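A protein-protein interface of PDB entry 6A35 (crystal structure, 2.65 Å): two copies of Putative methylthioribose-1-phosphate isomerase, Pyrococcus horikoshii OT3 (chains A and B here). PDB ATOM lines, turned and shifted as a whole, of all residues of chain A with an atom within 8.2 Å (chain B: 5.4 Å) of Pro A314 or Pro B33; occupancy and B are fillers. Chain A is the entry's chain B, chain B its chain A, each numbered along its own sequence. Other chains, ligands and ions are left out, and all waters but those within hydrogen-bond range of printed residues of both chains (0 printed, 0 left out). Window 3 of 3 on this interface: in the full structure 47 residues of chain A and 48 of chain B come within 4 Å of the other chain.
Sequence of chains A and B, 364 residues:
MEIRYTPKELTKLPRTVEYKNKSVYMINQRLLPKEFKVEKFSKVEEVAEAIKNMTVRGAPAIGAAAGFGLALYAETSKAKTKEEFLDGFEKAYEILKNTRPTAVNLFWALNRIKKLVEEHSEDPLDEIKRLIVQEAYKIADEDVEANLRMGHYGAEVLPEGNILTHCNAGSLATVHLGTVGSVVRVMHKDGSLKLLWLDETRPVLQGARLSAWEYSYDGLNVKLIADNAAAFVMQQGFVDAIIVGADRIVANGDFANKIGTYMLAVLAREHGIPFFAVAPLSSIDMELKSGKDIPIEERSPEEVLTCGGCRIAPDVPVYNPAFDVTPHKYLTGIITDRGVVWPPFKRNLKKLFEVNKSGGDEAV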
ATOM      1  N   PRO A 301     -15.971 -26.591 -15.590  1.00  0.00           N
ATOM      2  CA  PRO A 301     -15.050 -25.961 -16.546  1.00  0.00           C
ATOM      3  C   PRO A 301     -13.671 -25.772 -15.949  1.00  0.00           C
ATOM      4  O   PRO A 301     -12.688 -25.629 -16.681  1.00  0.00           O
ATOM      5  CB  PRO A 301     -15.687 -24.615 -16.831  1.00  0.00           C
ATOM      6  CG  PRO A 301     -17.145 -24.776 -16.477  1.00  0.00           C
ATOM      7  CD  PRO A 301     -17.259 -25.877 -15.470  1.00  0.00           C
ATOM      8  N   VAL A 304     -10.541 -27.934 -16.958  1.00  0.00           N
ATOM      9  CA  VAL A 304      -9.862 -27.576 -18.207  1.00  0.00           C
ATOM     10  C   VAL A 304      -9.148 -26.252 -18.047  1.00  0.00           C
ATOM     11  O   VAL A 304      -7.985 -26.126 -18.408  1.00  0.00           O
ATOM     12  CB  VAL A 304     -10.860 -27.449 -19.386  1.00  0.00           C
ATOM     13  CG1 VAL A 304     -10.176 -26.875 -20.600  1.00  0.00           C
ATOM     14  CG2 VAL A 304     -11.471 -28.800 -19.705  1.00  0.00           C
ATOM     15  N   LEU A 305      -9.867 -25.269 -17.524  1.00  0.00           N
ATOM     16  CA  LEU A 305      -9.309 -23.968 -17.172  1.00  0.00           C
ATOM     17  C   LEU A 305      -8.051 -24.008 -16.336  1.00  0.00           C
ATOM     18  O   LEU A 305      -7.240 -23.094 -16.418  1.00  0.00           O
ATOM     19  CB  LEU A 305     -10.366 -23.143 -16.422  1.00  0.00           C
ATOM     20  CG  LEU A 305     -11.558 -22.632 -17.259  1.00  0.00           C
ATOM     21  CD1 LEU A 305     -12.283 -21.491 -16.549  1.00  0.00           C
ATOM     22  CD2 LEU A 305     -11.136 -22.185 -18.652  1.00  0.00           C
ATOM     23  N   ARG A 311      -3.981 -22.095 -12.846  1.00  0.00           N
ATOM     24  CA  ARG A 311      -4.811 -21.674 -13.946  1.00  0.00           C
ATOM     25  C   ARG A 311      -3.926 -21.526 -15.195  1.00  0.00           C
ATOM     26  O   ARG A 311      -2.769 -21.089 -15.104  1.00  0.00           O
ATOM     27  CB  ARG A 311      -5.477 -20.323 -13.630  1.00  0.00           C
ATOM     28  CG  ARG A 311      -6.443 -19.822 -14.700  1.00  0.00           C
ATOM     29  CD  ARG A 311      -7.444 -18.839 -14.114  1.00  0.00           C
ATOM     30  NE  ARG A 311      -7.947 -19.333 -12.828  1.00  0.00           N
ATOM     31  CZ  ARG A 311      -9.008 -20.122 -12.657  1.00  0.00           C
ATOM     32  NH1 ARG A 311      -9.767 -20.517 -13.678  1.00  0.00           N
ATOM     33  NH2 ARG A 311      -9.315 -20.504 -11.433  1.00  0.00           N
ATOM     34  N   ILE A 312      -4.480 -21.885 -16.352  1.00  0.00           N
ATOM     35  CA  ILE A 312      -3.751 -21.808 -17.601  1.00  0.00           C
ATOM     36  C   ILE A 312      -4.584 -21.189 -18.699  1.00  0.00           C
ATOM     37  O   ILE A 312      -4.174 -21.202 -19.838  1.00  0.00           O
ATOM     38  CB  ILE A 312      -3.205 -23.182 -18.028  1.00  0.00           C
ATOM     39  CG1 ILE A 312      -4.246 -24.278 -17.838  1.00  0.00           C
ATOM     40  CG2 ILE A 312      -1.981 -23.550 -17.203  1.00  0.00           C
ATOM     41  CD1 ILE A 312      -5.208 -24.438 -18.993  1.00  0.00           C
ATOM     42  N   ALA A 313      -5.717 -20.592 -18.368  1.00  0.00           N
ATOM     43  CA  ALA A 313      -6.583 -20.045 -19.388  1.00  0.00           C
ATOM     44  C   ALA A 313      -7.346 -18.815 -18.921  1.00  0.00           C
ATOM     45  O   ALA A 313      -7.485 -18.579 -17.713  1.00  0.00           O
ATOM     46  CB  ALA A 313      -7.554 -21.096 -19.867  1.00  0.00           C
ATOM     47  N   PRO A 314      -7.792 -17.978 -19.886  1.00  0.00           N
ATOM     48  CA  PRO A 314      -8.698 -16.857 -19.600  1.00  0.00           C
ATOM     49  C   PRO A 314     -10.107 -17.399 -19.449  1.00  0.00           C
ATOM     50  O   PRO A 314     -10.370 -18.523 -19.896  1.00  0.00           O
ATOM     51  CB  PRO A 314      -8.616 -16.037 -20.873  1.00  0.00           C
ATOM     52  CG  PRO A 314      -8.401 -17.052 -21.931  1.00  0.00           C
ATOM     53  CD  PRO A 314      -7.417 -18.006 -21.315  1.00  0.00           C
ATOM     54  N   ASP A 315     -11.018 -16.638 -18.865  1.00  0.00           N
ATOM     55  CA  ASP A 315     -12.359 -17.182 -18.685  1.00  0.00           C
ATOM     56  C   ASP A 315     -13.155 -17.098 -19.992  1.00  0.00           C
ATOM     57  O   ASP A 315     -13.648 -16.036 -20.395  1.00  0.00           O
ATOM     58  CB  ASP A 315     -13.072 -16.634 -17.440  1.00  0.00           C
ATOM     59  CG  ASP A 315     -12.811 -17.524 -16.172  1.00  0.00           C
ATOM     60  OD1 ASP A 315     -11.639 -17.978 -15.961  1.00  0.00           O
ATOM     61  OD2 ASP A 315     -13.788 -17.788 -15.416  1.00  0.00           O
ATOM     62  N   VAL A 316     -13.198 -18.269 -20.648  1.00  0.00           N
ATOM     63  CA  VAL A 316     -13.869 -18.518 -21.936  1.00  0.00           C
ATOM     64  C   VAL A 316     -14.726 -19.759 -21.740  1.00  0.00           C
ATOM     65  O   VAL A 316     -14.360 -20.598 -20.917  1.00  0.00           O
ATOM     66  CB  VAL A 316     -12.846 -18.798 -23.090  1.00  0.00           C
ATOM     67  CG1 VAL A 316     -12.118 -17.521 -23.501  1.00  0.00           C
ATOM     68  CG2 VAL A 316     -11.811 -19.855 -22.716  1.00  0.00           C
ATOM     69  N   PRO A 317     -15.827 -19.905 -22.514  1.00  0.00           N
ATOM     70  CA  PRO A 317     -16.643 -21.138 -22.469  1.00  0.00           C
ATOM     71  C   PRO A 317     -15.786 -22.366 -22.633  1.00  0.00           C
ATOM     72  O   PRO A 317     -14.747 -22.280 -23.273  1.00  0.00           O
ATOM     73  CB  PRO A 317     -17.579 -21.020 -23.668  1.00  0.00           C
ATOM     74  CG  PRO A 317     -17.575 -19.561 -24.060  1.00  0.00           C
ATOM     75  CD  PRO A 317     -16.242 -19.009 -23.620  1.00  0.00           C
ATOM     76  N   VAL A 318     -16.221 -23.490 -22.047  1.00  0.00           N
ATOM     77  CA  VAL A 318     -15.529 -24.786 -22.131  1.00  0.00           C
ATOM     78  C   VAL A 318     -16.486 -25.946 -22.438  1.00  0.00           C
ATOM     79  O   VAL A 318     -17.659 -25.890 -22.152  1.00  0.00           O
ATOM     80  CB  VAL A 318     -14.814 -25.091 -20.789  1.00  0.00           C
ATOM     81  CG1 VAL A 318     -14.254 -26.535 -20.714  1.00  0.00           C
ATOM     82  CG2 VAL A 318     -13.720 -24.075 -20.555  1.00  0.00           C
ATOM     83  N   LEU B  31       3.261 -13.032 -20.421  1.00  0.00           N
ATOM     84  CA  LEU B  31       2.236 -12.587 -19.455  1.00  0.00           C
ATOM     85  C   LEU B  31       0.800 -12.999 -19.782  1.00  0.00           C
ATOM     86  O   LEU B  31      -0.143 -12.683 -19.053  1.00  0.00           O
ATOM     87  CB  LEU B  31       2.263 -11.067 -19.312  1.00  0.00           C
ATOM     88  CG  LEU B  31       3.509 -10.428 -18.699  1.00  0.00           C
ATOM     89  CD1 LEU B  31       3.308  -8.913 -18.607  1.00  0.00           C
ATOM     90  CD2 LEU B  31       3.821 -11.052 -17.349  1.00  0.00           C
ATOM     91  N   LEU B  32       0.623 -13.701 -20.876  1.00  0.00           N
ATOM     92  CA  LEU B  32      -0.694 -14.117 -21.259  1.00  0.00           C
ATOM     93  C   LEU B  32      -1.026 -15.502 -20.624  1.00  0.00           C
ATOM     94  O   LEU B  32      -0.095 -16.319 -20.349  1.00  0.00           O
ATOM     95  CB  LEU B  32      -0.764 -14.146 -22.792  1.00  0.00           C
ATOM     96  CG  LEU B  32      -0.767 -12.804 -23.548  1.00  0.00           C
ATOM     97  CD1 LEU B  32      -0.414 -13.027 -25.006  1.00  0.00           C
ATOM     98  CD2 LEU B  32      -2.125 -12.137 -23.466  1.00  0.00           C
ATOM     99  N   PRO B  33      -2.319 -15.786 -20.376  1.00  0.00           N
ATOM    100  CA  PRO B  33      -3.472 -14.891 -20.587  1.00  0.00           C
ATOM    101  C   PRO B  33      -3.795 -13.954 -19.419  1.00  0.00           C
ATOM    102  O   PRO B  33      -4.683 -13.105 -19.546  1.00  0.00           O
ATOM    103  CB  PRO B  33      -4.634 -15.879 -20.691  1.00  0.00           C
ATOM    104  CG  PRO B  33      -4.253 -16.989 -19.791  1.00  0.00           C
ATOM    105  CD  PRO B  33      -2.772 -17.147 -20.035  1.00  0.00           C
ATOM    106  N   LYS B  34      -3.112 -14.154 -18.285  1.00  0.00           N
ATOM    107  CA  LYS B  34      -3.321 -13.349 -17.056  1.00  0.00           C
ATOM    108  C   LYS B  34      -3.342 -11.825 -17.326  1.00  0.00           C
ATOM    109  O   LYS B  34      -4.222 -11.099 -16.893  1.00  0.00           O
ATOM    110  CB  LYS B  34      -2.191 -13.667 -16.063  1.00  0.00           C
ATOM    111  CG  LYS B  34      -2.557 -13.633 -14.584  1.00  0.00           C
ATOM    112  CD  LYS B  34      -1.409 -14.258 -13.774  1.00  0.00           C
ATOM    113  CE  LYS B  34      -1.839 -14.880 -12.446  1.00  0.00           C
ATOM    114  NZ  LYS B  34      -1.991 -13.879 -11.353  1.00  0.00           N
ATOM    115  N   GLU B  35      -2.346 -11.354 -18.050  1.00  0.00           N
ATOM    116  CA  GLU B  35      -2.094  -9.936 -18.127  1.00  0.00           C
ATOM    117  C   GLU B  35      -1.645  -9.631 -19.528  1.00  0.00           C
ATOM    118  O   GLU B  35      -0.742 -10.291 -20.067  1.00  0.00           O
ATOM    119  CB  GLU B  35      -1.025  -9.555 -17.111  1.00  0.00           C
ATOM    120  CG  GLU B  35      -0.962  -8.093 -16.725  1.00  0.00           C
ATOM    121  CD  GLU B  35       0.452  -7.675 -16.308  1.00  0.00           C
ATOM    122  OE1 GLU B  35       1.120  -8.456 -15.557  1.00  0.00           O
ATOM    123  OE2 GLU B  35       0.888  -6.572 -16.750  1.00  0.00           O
ATOM    124  N   PHE B  36      -2.325  -8.656 -20.121  1.00  0.00           N
ATOM    125  CA  PHE B  36      -2.033  -8.196 -21.472  1.00  0.00           C
ATOM    126  C   PHE B  36      -1.178  -6.945 -21.340  1.00  0.00           C
ATOM    127  O   PHE B  36      -1.603  -5.950 -20.752  1.00  0.00           O
ATOM    128  CB  PHE B  36      -3.338  -7.913 -22.228  1.00  0.00           C
ATOM    129  CG  PHE B  36      -3.155  -7.206 -23.561  1.00  0.00           C
ATOM    130  CD1 PHE B  36      -1.996  -7.361 -24.323  1.00  0.00           C
ATOM    131  CD2 PHE B  36      -4.175  -6.415 -24.078  1.00  0.00           C
ATOM    132  CE1 PHE B  36      -1.861  -6.723 -25.542  1.00  0.00           C
ATOM    133  CE2 PHE B  36      -4.043  -5.788 -25.307  1.00  0.00           C
ATOM    134  CZ  PHE B  36      -2.880  -5.946 -26.036  1.00  0.00           C
ATOM    135  N   ALA B 208      -4.843 -22.955 -25.049  1.00  0.00           N
ATOM    136  CA  ALA B 208      -5.526 -22.363 -23.911  1.00  0.00           C
ATOM    137  C   ALA B 208      -5.009 -20.957 -23.695  1.00  0.00           C
ATOM    138  O   ALA B 208      -5.779 -19.995 -23.696  1.00  0.00           O
ATOM    139  CB  ALA B 208      -5.309 -23.209 -22.657  1.00  0.00           C
ATOM    140  N   ARG B 209      -3.689 -20.870 -23.560  1.00  0.00           N
ATOM    141  CA  ARG B 209      -2.995 -19.702 -23.012  1.00  0.00           C
ATOM    142  C   ARG B 209      -3.027 -18.486 -23.989  1.00  0.00           C
ATOM    143  O   ARG B 209      -3.241 -17.367 -23.568  1.00  0.00           O
ATOM    144  CB  ARG B 209      -1.557 -20.119 -22.705  1.00  0.00           C
ATOM    145  CG  ARG B 209      -0.953 -19.495 -21.484  1.00  0.00           C
ATOM    146  CD  ARG B 209       0.145 -20.377 -20.920  1.00  0.00           C
ATOM    147  NE  ARG B 209       1.112 -20.746 -21.932  1.00  0.00           N
ATOM    148  CZ  ARG B 209       2.023 -19.925 -22.453  1.00  0.00           C
ATOM    149  NH1 ARG B 209       2.117 -18.633 -22.090  1.00  0.00           N
ATOM    150  NH2 ARG B 209       2.849 -20.409 -23.359  1.00  0.00           N
ATOM    151  N   ALA B 212      -7.030 -18.795 -27.025  1.00  0.00           N
ATOM    152  CA  ALA B 212      -8.364 -18.553 -26.468  1.00  0.00           C
ATOM    153  C   ALA B 212      -8.412 -17.146 -26.007  1.00  0.00           C
ATOM    154  O   ALA B 212      -9.471 -16.547 -25.921  1.00  0.00           O
ATOM    155  CB  ALA B 212      -8.652 -19.488 -25.309  1.00  0.00           C
ATOM    156  N   TRP B 213      -7.252 -16.612 -25.678  1.00  0.00           N
ATOM    157  CA  TRP B 213      -7.191 -15.248 -25.244  1.00  0.00           C
ATOM    158  C   TRP B 213      -7.411 -14.295 -26.462  1.00  0.00           C
ATOM    159  O   TRP B 213      -8.313 -13.461 -26.436  1.00  0.00           O
ATOM    160  CB  TRP B 213      -5.883 -14.991 -24.515  1.00  0.00           C
ATOM    161  CG  TRP B 213      -5.763 -13.561 -24.140  1.00  0.00           C
ATOM    162  CD1 TRP B 213      -6.198 -12.970 -22.994  1.00  0.00           C
ATOM    163  CD2 TRP B 213      -5.201 -12.525 -24.944  1.00  0.00           C
ATOM    164  NE1 TRP B 213      -5.931 -11.629 -23.035  1.00  0.00           N
ATOM    165  CE2 TRP B 213      -5.319 -11.331 -24.219  1.00  0.00           C
ATOM    166  CE3 TRP B 213      -4.586 -12.501 -26.200  1.00  0.00           C
ATOM    167  CZ2 TRP B 213      -4.864 -10.131 -24.700  1.00  0.00           C
ATOM    168  CZ3 TRP B 213      -4.130 -11.311 -26.672  1.00  0.00           C
ATOM    169  CH2 TRP B 213      -4.277 -10.134 -25.930  1.00  0.00           C
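The backbone carbonyl oxygen (O) of Leu A305 lies within hydrogen-bond range of the backbone NH (N) of Ile A312, at 3.0 Å.
O of Ile A312 touches CB of Ala B208 (3.6 Å).
Ile A312 touches Arg B209 (O to CA, 3.7 Å).
C of Ala A313 touches CG of Pro B33, 3.7 Å away.
Pro A314 touches Pro B33 (CD to CB, 3.6 Å).
Ala B208 touches Pro A314 (O to CD, 3.5 Å).
Trp B213 touches Pro A314 (N to CG, 3.9 Å).
Ala B212 touches Val A316.
Of the printed residues of chain B, Ile A312 touches Ala B208 (3.6 Å) and Arg B209 (3.7 Å).
Printed residues of chain A within 4 Å of Trp B213: Pro A314 (3.9 Å).
Of the printed residues of chain B, Ala A313 touches Pro B33 (3.7 Å).
Of the printed residues of chain B, Val A316 touches Ala B212.
Of the printed residues of chain A, Ala B208 touches Ile A312 (3.6 Å) and Pro A314 (3.5 Å).
Asp A315 touches none of the printed residues of chain B.
The nearest residue of chain B that does not touch Pro A314 is Ala B212 (4.1 Å).
The nearest residue of chain A that does not touch Pro B33 is Ile A312 (4.2 Å).
Of the 10 printed residues of chain B, 5 touch a printed residue of chain A.
Hydrophobic or aromatic side chains of chain B that line the printed part of chain A: Pro B33 and Ala B208.
Of the 11 printed residues of chain A, 4 touch a printed residue of chain B.
Hydrophobic or aromatic side chains of chain A within 4 Å of the printed part of chain B: Ile A312, Pro A314 and Val A316.
Along chain A the printed residues that touch a printed residue of chain B span positions 312 to 316.
Among the printed residues, 7 pairs touch across the chains.
Among the printed residues, no Asp or Glu carboxylate lies within 4 Å of a Lys or Arg side-chain nitrogen of the other chain.
No position is printed for both chains.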
